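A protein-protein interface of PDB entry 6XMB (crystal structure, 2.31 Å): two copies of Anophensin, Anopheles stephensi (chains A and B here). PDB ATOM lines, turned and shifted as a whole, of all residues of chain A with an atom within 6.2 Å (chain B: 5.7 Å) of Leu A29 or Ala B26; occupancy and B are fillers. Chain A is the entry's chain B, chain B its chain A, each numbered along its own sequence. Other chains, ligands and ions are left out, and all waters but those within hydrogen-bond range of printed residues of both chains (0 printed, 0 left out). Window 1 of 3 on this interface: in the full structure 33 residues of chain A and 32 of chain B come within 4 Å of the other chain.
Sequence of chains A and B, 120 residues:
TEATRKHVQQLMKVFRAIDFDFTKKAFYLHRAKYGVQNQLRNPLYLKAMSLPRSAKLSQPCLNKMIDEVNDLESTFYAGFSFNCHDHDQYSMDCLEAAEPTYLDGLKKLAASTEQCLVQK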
ATOM      1  N   LYS A  24      21.601  28.851  10.307  1.00  0.00           N
ATOM      2  CA  LYS A  24      20.898  27.945  11.217  1.00  0.00           C
ATOM      3  C   LYS A  24      21.785  26.766  11.613  1.00  0.00           C
ATOM      4  O   LYS A  24      21.855  26.409  12.789  1.00  0.00           O
ATOM      5  CB  LYS A  24      19.586  27.447  10.590  1.00  0.00           C
ATOM      6  CG  LYS A  24      18.475  28.494  10.523  1.00  0.00           C
ATOM      7  CD  LYS A  24      17.112  27.900  10.135  1.00  0.00           C
ATOM      8  CE  LYS A  24      17.093  27.374   8.710  1.00  0.00           C
ATOM      9  NZ  LYS A  24      15.855  27.792   7.949  1.00  0.00           N
ATOM     10  N   LYS A  25      22.502  26.174  10.653  1.00  0.00           N
ATOM     11  CA  LYS A  25      23.424  25.097  11.004  1.00  0.00           C
ATOM     12  C   LYS A  25      24.544  25.580  11.930  1.00  0.00           C
ATOM     13  O   LYS A  25      25.008  24.812  12.779  1.00  0.00           O
ATOM     14  CB  LYS A  25      24.028  24.466   9.748  1.00  0.00           C
ATOM     15  CG  LYS A  25      23.035  23.866   8.710  1.00  0.00           C
ATOM     16  CD  LYS A  25      23.801  22.924   7.744  1.00  0.00           C
ATOM     17  CE  LYS A  25      23.301  22.935   6.305  1.00  0.00           C
ATOM     18  NZ  LYS A  25      21.925  22.432   6.213  1.00  0.00           N
ATOM     19  N   ALA A  26      24.992  26.840  11.793  1.00  0.00           N
ATOM     20  CA  ALA A  26      26.028  27.343  12.694  1.00  0.00           C
ATOM     21  C   ALA A  26      25.464  27.619  14.080  1.00  0.00           C
ATOM     22  O   ALA A  26      26.163  27.468  15.078  1.00  0.00           O
ATOM     23  CB  ALA A  26      26.679  28.613  12.125  1.00  0.00           C
ATOM     24  N   PHE A  27      24.210  28.063  14.155  1.00  0.00           N
ATOM     25  CA  PHE A  27      23.574  28.241  15.450  1.00  0.00           C
ATOM     26  C   PHE A  27      23.397  26.900  16.155  1.00  0.00           C
ATOM     27  O   PHE A  27      23.668  26.783  17.354  1.00  0.00           O
ATOM     28  CB  PHE A  27      22.238  28.946  15.282  1.00  0.00           C
ATOM     29  CG  PHE A  27      21.532  29.203  16.575  1.00  0.00           C
ATOM     30  CD1 PHE A  27      21.916  30.253  17.386  1.00  0.00           C
ATOM     31  CD2 PHE A  27      20.482  28.400  16.972  1.00  0.00           C
ATOM     32  CE1 PHE A  27      21.272  30.503  18.572  1.00  0.00           C
ATOM     33  CE2 PHE A  27      19.825  28.643  18.162  1.00  0.00           C
ATOM     34  CZ  PHE A  27      20.220  29.696  18.964  1.00  0.00           C
ATOM     35  N   TYR A  28      22.975  25.870  15.417  1.00  0.00           N
ATOM     36  CA  TYR A  28      22.970  24.517  15.965  1.00  0.00           C
ATOM     37  C   TYR A  28      24.309  24.181  16.601  1.00  0.00           C
ATOM     38  O   TYR A  28      24.372  23.687  17.730  1.00  0.00           O
ATOM     39  CB  TYR A  28      22.653  23.472  14.882  1.00  0.00           C
ATOM     40  CG  TYR A  28      23.167  22.110  15.297  1.00  0.00           C
ATOM     41  CD1 TYR A  28      22.454  21.330  16.194  1.00  0.00           C
ATOM     42  CD2 TYR A  28      24.397  21.638  14.849  1.00  0.00           C
ATOM     43  CE1 TYR A  28      22.938  20.111  16.625  1.00  0.00           C
ATOM     44  CE2 TYR A  28      24.899  20.433  15.273  1.00  0.00           C
ATOM     45  CZ  TYR A  28      24.153  19.670  16.169  1.00  0.00           C
ATOM     46  OH  TYR A  28      24.619  18.460  16.602  1.00  0.00           O
ATOM     47  N   LEU A  29      25.392  24.410  15.861  1.00  0.00           N
ATOM     48  CA  LEU A  29      26.719  23.986  16.294  1.00  0.00           C
ATOM     49  C   LEU A  29      27.141  24.711  17.560  1.00  0.00           C
ATOM     50  O   LEU A  29      27.748  24.110  18.450  1.00  0.00           O
ATOM     51  CB  LEU A  29      27.720  24.234  15.164  1.00  0.00           C
ATOM     52  CG  LEU A  29      28.957  23.338  15.102  1.00  0.00           C
ATOM     53  CD1 LEU A  29      28.568  21.866  14.929  1.00  0.00           C
ATOM     54  CD2 LEU A  29      29.908  23.804  13.985  1.00  0.00           C
ATOM     55  N   HIS A  30      26.824  26.006  17.660  1.00  0.00           N
ATOM     56  CA  HIS A  30      27.064  26.742  18.905  1.00  0.00           C
ATOM     57  C   HIS A  30      26.260  26.145  20.063  1.00  0.00           C
ATOM     58  O   HIS A  30      26.789  25.943  21.166  1.00  0.00           O
ATOM     59  CB  HIS A  30      26.715  28.230  18.728  1.00  0.00           C
ATOM     60  CG  HIS A  30      27.784  29.055  18.077  1.00  0.00           C
ATOM     61  ND1 HIS A  30      27.744  29.425  16.743  1.00  0.00           N
ATOM     62  CD2 HIS A  30      28.911  29.614  18.586  1.00  0.00           C
ATOM     63  CE1 HIS A  30      28.801  30.165  16.460  1.00  0.00           C
ATOM     64  NE2 HIS A  30      29.526  30.297  17.561  1.00  0.00           N
ATOM     65  N   ARG A  31      24.977  25.821  19.823  1.00  0.00           N
ATOM     66  CA  ARG A  31      24.155  25.197  20.873  1.00  0.00           C
ATOM     67  C   ARG A  31      24.747  23.873  21.319  1.00  0.00           C
ATOM     68  O   ARG A  31      24.819  23.597  22.514  1.00  0.00           O
ATOM     69  CB  ARG A  31      22.715  24.995  20.397  1.00  0.00           C
ATOM     70  CG  ARG A  31      21.948  26.278  20.109  1.00  0.00           C
ATOM     71  CD  ARG A  31      21.721  27.106  21.364  1.00  0.00           C
ATOM     72  NE  ARG A  31      20.826  26.420  22.287  1.00  0.00           N
ATOM     73  CZ  ARG A  31      20.230  26.999  23.326  1.00  0.00           C
ATOM     74  NH1 ARG A  31      20.415  28.290  23.563  1.00  0.00           N
ATOM     75  NH2 ARG A  31      19.441  26.283  24.119  1.00  0.00           N
ATOM     76  N   ALA A  32      25.215  23.054  20.382  1.00  0.00           N
ATOM     77  CA  ALA A  32      25.873  21.815  20.768  1.00  0.00           C
ATOM     78  C   ALA A  32      27.165  22.083  21.531  1.00  0.00           C
ATOM     79  O   ALA A  32      27.521  21.331  22.445  1.00  0.00           O
ATOM     80  CB  ALA A  32      26.155  20.963  19.540  1.00  0.00           C
ATOM     81  N   LYS A  33      27.890  23.144  21.168  1.00  0.00           N
ATOM     82  CA  LYS A  33      29.110  23.466  21.890  1.00  0.00           C
ATOM     83  C   LYS A  33      28.793  23.886  23.310  1.00  0.00           C
ATOM     84  O   LYS A  33      29.383  23.371  24.266  1.00  0.00           O
ATOM     85  CB  LYS A  33      29.891  24.571  21.159  1.00  0.00           C
ATOM     86  CG  LYS A  33      31.307  24.794  21.705  1.00  0.00           C
ATOM     87  CD  LYS A  33      32.074  25.866  20.909  1.00  0.00           C
ATOM     88  CE  LYS A  33      32.099  27.233  21.607  1.00  0.00           C
ATOM     89  NZ  LYS A  33      32.886  28.252  20.809  1.00  0.00           N
ATOM     90  N   TYR A  34      27.852  24.814  23.476  1.00  0.00           N
ATOM     91  CA  TYR A  34      27.544  25.252  24.830  1.00  0.00           C
ATOM     92  C   TYR A  34      26.804  24.177  25.606  1.00  0.00           C
ATOM     93  O   TYR A  34      26.718  24.265  26.835  1.00  0.00           O
ATOM     94  CB  TYR A  34      26.758  26.570  24.800  1.00  0.00           C
ATOM     95  CG  TYR A  34      27.636  27.798  24.508  1.00  0.00           C
ATOM     96  CD1 TYR A  34      28.159  28.583  25.544  1.00  0.00           C
ATOM     97  CD2 TYR A  34      27.949  28.170  23.195  1.00  0.00           C
ATOM     98  CE1 TYR A  34      28.956  29.707  25.272  1.00  0.00           C
ATOM     99  CE2 TYR A  34      28.744  29.283  22.922  1.00  0.00           C
ATOM    100  CZ  TYR A  34      29.248  30.048  23.962  1.00  0.00           C
ATOM    101  OH  TYR A  34      30.041  31.159  23.689  1.00  0.00           O
ATOM    102  N   GLU A  73      26.554  14.023  19.784  1.00  0.00           N
ATOM    103  CA  GLU A  73      26.374  15.146  18.876  1.00  0.00           C
ATOM    104  C   GLU A  73      25.978  14.669  17.485  1.00  0.00           C
ATOM    105  O   GLU A  73      25.207  15.337  16.792  1.00  0.00           O
ATOM    106  CB  GLU A  73      27.646  16.006  18.830  1.00  0.00           C
ATOM    107  CG  GLU A  73      27.451  17.343  18.133  1.00  0.00           C
ATOM    108  CD  GLU A  73      27.568  17.234  16.613  1.00  0.00           C
ATOM    109  OE1 GLU A  73      26.789  17.921  15.904  1.00  0.00           O
ATOM    110  OE2 GLU A  73      28.431  16.450  16.145  1.00  0.00           O
ATOM    111  N   ASP B  21      37.471  20.062  18.003  1.00  0.00           N
ATOM    112  CA  ASP B  21      36.519  19.298  17.178  1.00  0.00           C
ATOM    113  C   ASP B  21      35.381  20.177  16.699  1.00  0.00           C
ATOM    114  O   ASP B  21      35.039  20.172  15.518  1.00  0.00           O
ATOM    115  CB  ASP B  21      35.924  18.116  17.942  1.00  0.00           C
ATOM    116  CG  ASP B  21      36.807  16.889  17.929  1.00  0.00           C
ATOM    117  OD1 ASP B  21      37.847  16.893  17.243  1.00  0.00           O
ATOM    118  OD2 ASP B  21      36.446  15.909  18.627  1.00  0.00           O
ATOM    119  N   PHE B  22      34.784  20.953  17.604  1.00  0.00           N
ATOM    120  CA  PHE B  22      33.751  21.895  17.187  1.00  0.00           C
ATOM    121  C   PHE B  22      34.294  22.917  16.197  1.00  0.00           C
ATOM    122  O   PHE B  22      33.590  23.307  15.259  1.00  0.00           O
ATOM    123  CB  PHE B  22      33.135  22.592  18.400  1.00  0.00           C
ATOM    124  CG  PHE B  22      32.135  21.732  19.132  1.00  0.00           C
ATOM    125  CD1 PHE B  22      30.945  21.387  18.531  1.00  0.00           C
ATOM    126  CD2 PHE B  22      32.402  21.258  20.402  1.00  0.00           C
ATOM    127  CE1 PHE B  22      30.044  20.601  19.158  1.00  0.00           C
ATOM    128  CE2 PHE B  22      31.490  20.460  21.046  1.00  0.00           C
ATOM    129  CZ  PHE B  22      30.304  20.128  20.421  1.00  0.00           C
ATOM    130  N   THR B  23      35.543  23.353  16.374  1.00  0.00           N
ATOM    131  CA  THR B  23      36.129  24.298  15.427  1.00  0.00           C
ATOM    132  C   THR B  23      36.210  23.684  14.037  1.00  0.00           C
ATOM    133  O   THR B  23      35.822  24.305  13.054  1.00  0.00           O
ATOM    134  CB  THR B  23      37.523  24.745  15.879  1.00  0.00           C
ATOM    135  OG1 THR B  23      37.403  25.717  16.907  1.00  0.00           O
ATOM    136  CG2 THR B  23      38.272  25.399  14.687  1.00  0.00           C
ATOM    137  N   LYS B  24      36.724  22.457  13.945  1.00  0.00           N
ATOM    138  CA  LYS B  24      36.805  21.768  12.666  1.00  0.00           C
ATOM    139  C   LYS B  24      35.428  21.639  12.004  1.00  0.00           C
ATOM    140  O   LYS B  24      35.297  21.784  10.779  1.00  0.00           O
ATOM    141  CB  LYS B  24      37.437  20.392  12.876  1.00  0.00           C
ATOM    142  CG  LYS B  24      38.902  20.411  12.577  1.00  0.00           C
ATOM    143  CD  LYS B  24      39.681  19.751  13.649  1.00  0.00           C
ATOM    144  CE  LYS B  24      39.674  18.256  13.500  1.00  0.00           C
ATOM    145  NZ  LYS B  24      40.116  17.688  14.808  1.00  0.00           N
ATOM    146  N   LYS B  25      34.391  21.392  12.795  1.00  0.00           N
ATOM    147  CA  LYS B  25      33.051  21.311  12.221  1.00  0.00           C
ATOM    148  C   LYS B  25      32.611  22.670  11.685  1.00  0.00           C
ATOM    149  O   LYS B  25      31.962  22.741  10.638  1.00  0.00           O
ATOM    150  CB  LYS B  25      32.069  20.766  13.266  1.00  0.00           C
ATOM    151  CG  LYS B  25      32.292  19.281  13.580  1.00  0.00           C
ATOM    152  CD  LYS B  25      31.523  18.778  14.846  1.00  0.00           C
ATOM    153  CE  LYS B  25      31.774  17.274  15.082  1.00  0.00           C
ATOM    154  NZ  LYS B  25      31.141  16.678  16.338  1.00  0.00           N
ATOM    155  N   ALA B  26      32.990  23.764  12.366  1.00  0.00           N
ATOM    156  CA  ALA B  26      32.639  25.095  11.880  1.00  0.00           C
ATOM    157  C   ALA B  26      33.412  25.439  10.612  1.00  0.00           C
ATOM    158  O   ALA B  26      32.907  26.187   9.760  1.00  0.00           O
ATOM    159  CB  ALA B  26      32.905  26.152  12.946  1.00  0.00           C
ATOM    160  N   PHE B  27      34.631  24.906  10.483  1.00  0.00           N
ATOM    161  CA  PHE B  27      35.387  25.044   9.244  1.00  0.00           C
ATOM    162  C   PHE B  27      34.691  24.315   8.095  1.00  0.00           C
ATOM    163  O   PHE B  27      34.630  24.839   6.978  1.00  0.00           O
ATOM    164  CB  PHE B  27      36.796  24.503   9.447  1.00  0.00           C
ATOM    165  CG  PHE B  27      37.684  24.677   8.277  1.00  0.00           C
ATOM    166  CD1 PHE B  27      38.081  25.940   7.869  1.00  0.00           C
ATOM    167  CD2 PHE B  27      38.168  23.581   7.591  1.00  0.00           C
ATOM    168  CE1 PHE B  27      38.923  26.111   6.786  1.00  0.00           C
ATOM    169  CE2 PHE B  27      39.025  23.758   6.494  1.00  0.00           C
ATOM    170  CZ  PHE B  27      39.398  25.022   6.112  1.00  0.00           C
ATOM    171  N   TYR B  28      34.173  23.102   8.357  1.00  0.00           N
ATOM    172  CA  TYR B  28      33.381  22.379   7.365  1.00  0.00           C
ATOM    173  C   TYR B  28      32.245  23.255   6.846  1.00  0.00           C
ATOM    174  O   TYR B  28      32.033  23.371   5.642  1.00  0.00           O
ATOM    175  CB  TYR B  28      32.800  21.065   7.947  1.00  0.00           C
ATOM    176  CG  TYR B  28      31.668  20.583   7.046  1.00  0.00           C
ATOM    177  CD1 TYR B  28      31.937  19.807   5.935  1.00  0.00           C
ATOM    178  CD2 TYR B  28      30.362  21.021   7.235  1.00  0.00           C
ATOM    179  CE1 TYR B  28      30.942  19.445   5.064  1.00  0.00           C
ATOM    180  CE2 TYR B  28      29.374  20.685   6.376  1.00  0.00           C
ATOM    181  CZ  TYR B  28      29.666  19.880   5.292  1.00  0.00           C
ATOM    182  OH  TYR B  28      28.676  19.536   4.415  1.00  0.00           O
ATOM    183  N   LEU B  29      31.483  23.865   7.757  1.00  0.00           N
ATOM    184  CA  LEU B  29      30.333  24.663   7.343  1.00  0.00           C
ATOM    185  C   LEU B  29      30.760  25.815   6.470  1.00  0.00           C
ATOM    186  O   LEU B  29      30.078  26.155   5.496  1.00  0.00           O
ATOM    187  CB  LEU B  29      29.603  25.210   8.558  1.00  0.00           C
ATOM    188  CG  LEU B  29      28.549  24.310   9.154  1.00  0.00           C
ATOM    189  CD1 LEU B  29      27.937  24.984  10.385  1.00  0.00           C
ATOM    190  CD2 LEU B  29      27.514  24.037   8.091  1.00  0.00           C
ATOM    191  N   HIS B  30      31.860  26.467   6.856  1.00  0.00           N
ATOM    192  CA  HIS B  30      32.378  27.599   6.115  1.00  0.00           C
ATOM    193  C   HIS B  30      32.755  27.184   4.697  1.00  0.00           C
ATOM    194  O   HIS B  30      32.377  27.845   3.732  1.00  0.00           O
ATOM    195  CB  HIS B  30      33.571  28.195   6.889  1.00  0.00           C
ATOM    196  CG  HIS B  30      34.577  28.908   6.033  1.00  0.00           C
ATOM    197  ND1 HIS B  30      34.391  30.198   5.572  1.00  0.00           N
ATOM    198  CD2 HIS B  30      35.794  28.521   5.574  1.00  0.00           C
ATOM    199  CE1 HIS B  30      35.446  30.572   4.864  1.00  0.00           C
ATOM    200  NE2 HIS B  30      36.312  29.572   4.849  1.00  0.00           N
ATOM    201  N   ARG B  31      33.491  26.081   4.552  1.00  0.00           N
ATOM    202  CA  ARG B  31      33.828  25.588   3.213  1.00  0.00           C
ATOM    203  C   ARG B  31      32.582  25.272   2.402  1.00  0.00           C
ATOM    204  O   ARG B  31      32.537  25.537   1.198  1.00  0.00           O
ATOM    205  CB  ARG B  31      34.692  24.327   3.311  1.00  0.00           C
ATOM    206  CG  ARG B  31      35.978  24.521   4.099  1.00  0.00           C
ATOM    207  CD  ARG B  31      36.893  25.531   3.388  1.00  0.00           C
ATOM    208  NE  ARG B  31      37.365  25.060   2.095  1.00  0.00           N
ATOM    209  CZ  ARG B  31      38.281  25.704   1.362  1.00  0.00           C
ATOM    210  NH1 ARG B  31      38.831  26.836   1.807  1.00  0.00           N
ATOM    211  NH2 ARG B  31      38.650  25.215   0.189  1.00  0.00           N
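The side-chain carboxylate of Glu A73 is in salt-bridge range of the side-chain amino group of Lys B25 (2.7 Å).
A ring nitrogen (ND1) of His A30 is in hydrogen-bond range of the backbone carbonyl oxygen (O) of Ala A26 (3.0 Å).
O of Glu A73 sits at hydrogen-bond distance from OH of Tyr A28, 3.2 Å away.
C of Lys A25 touches CD1 of Leu B29, 3.8 Å away.
N of Ala A26 touches CD1 of Leu B29, at 3.8 Å.
CD2 of Leu A29 touches O of Phe B22 (3.9 Å).
Lys B25 touches Leu A29.
Leu A29 touches Ala B26 (CD2 to N, 3.5 Å).
Ala A32 touches Phe B22.
CZ of Phe B22 touches CA of Lys A33, at 3.8 Å.
Of the printed residues of chain B, Lys A25 touches Leu B29.
Phe A27 touches none of the printed residues of chain B.
Leu A29 touches just these residues of chain B: Phe B22 (3.9 Å), Lys B25 (3.7 Å) and Ala B26 (3.5 Å).
Of the printed residues of chain B, Ala A32 touches Phe B22 (3.6 Å).
Tyr A34 touches none of the printed residues of chain B.
Printed residues of chain B within 4 Å of Glu A73: Lys B25 (2.7 Å).
Of chain A, only Leu A29 comes within 4 Å of Ala B26.
Printed residues of chain A within 4 Å of Leu B29: Lys A25 and Ala A26.
The nearest printed residue of chain A that does not touch Ala B26 is His A30 (6.7 Å).
Hydrophobic or aromatic side chains of chain A that line the printed part of chain B: Leu A29 and Ala A32.
Of the 11 printed residues of chain B, 4 touch a printed residue of chain A.
Hydrophobic or aromatic side chains of chain B that line the printed part of chain A: Phe B22, Ala B26 and Leu B29.
Among the printed residues, 8 pairs touch across the chains.
Among the printed residues, Asp or Glu carboxylates within 4 Å of a Lys or Arg side-chain nitrogen of the other chain: Glu A73 with Lys B25.
Lys A25 touches Leu B29, and with the chains exchanged Leu A29 touches Lys B25.
Ala A26 touches Leu B29, and with the chains exchanged Leu A29 touches Ala B26.
Positions printed for both chains: 24, 25, 26, 27, 28, 29, 30 and 31.
Of the 8 pairs that touch across the chains among the printed residues, 4 have their exchanged pair printed and touching as well.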
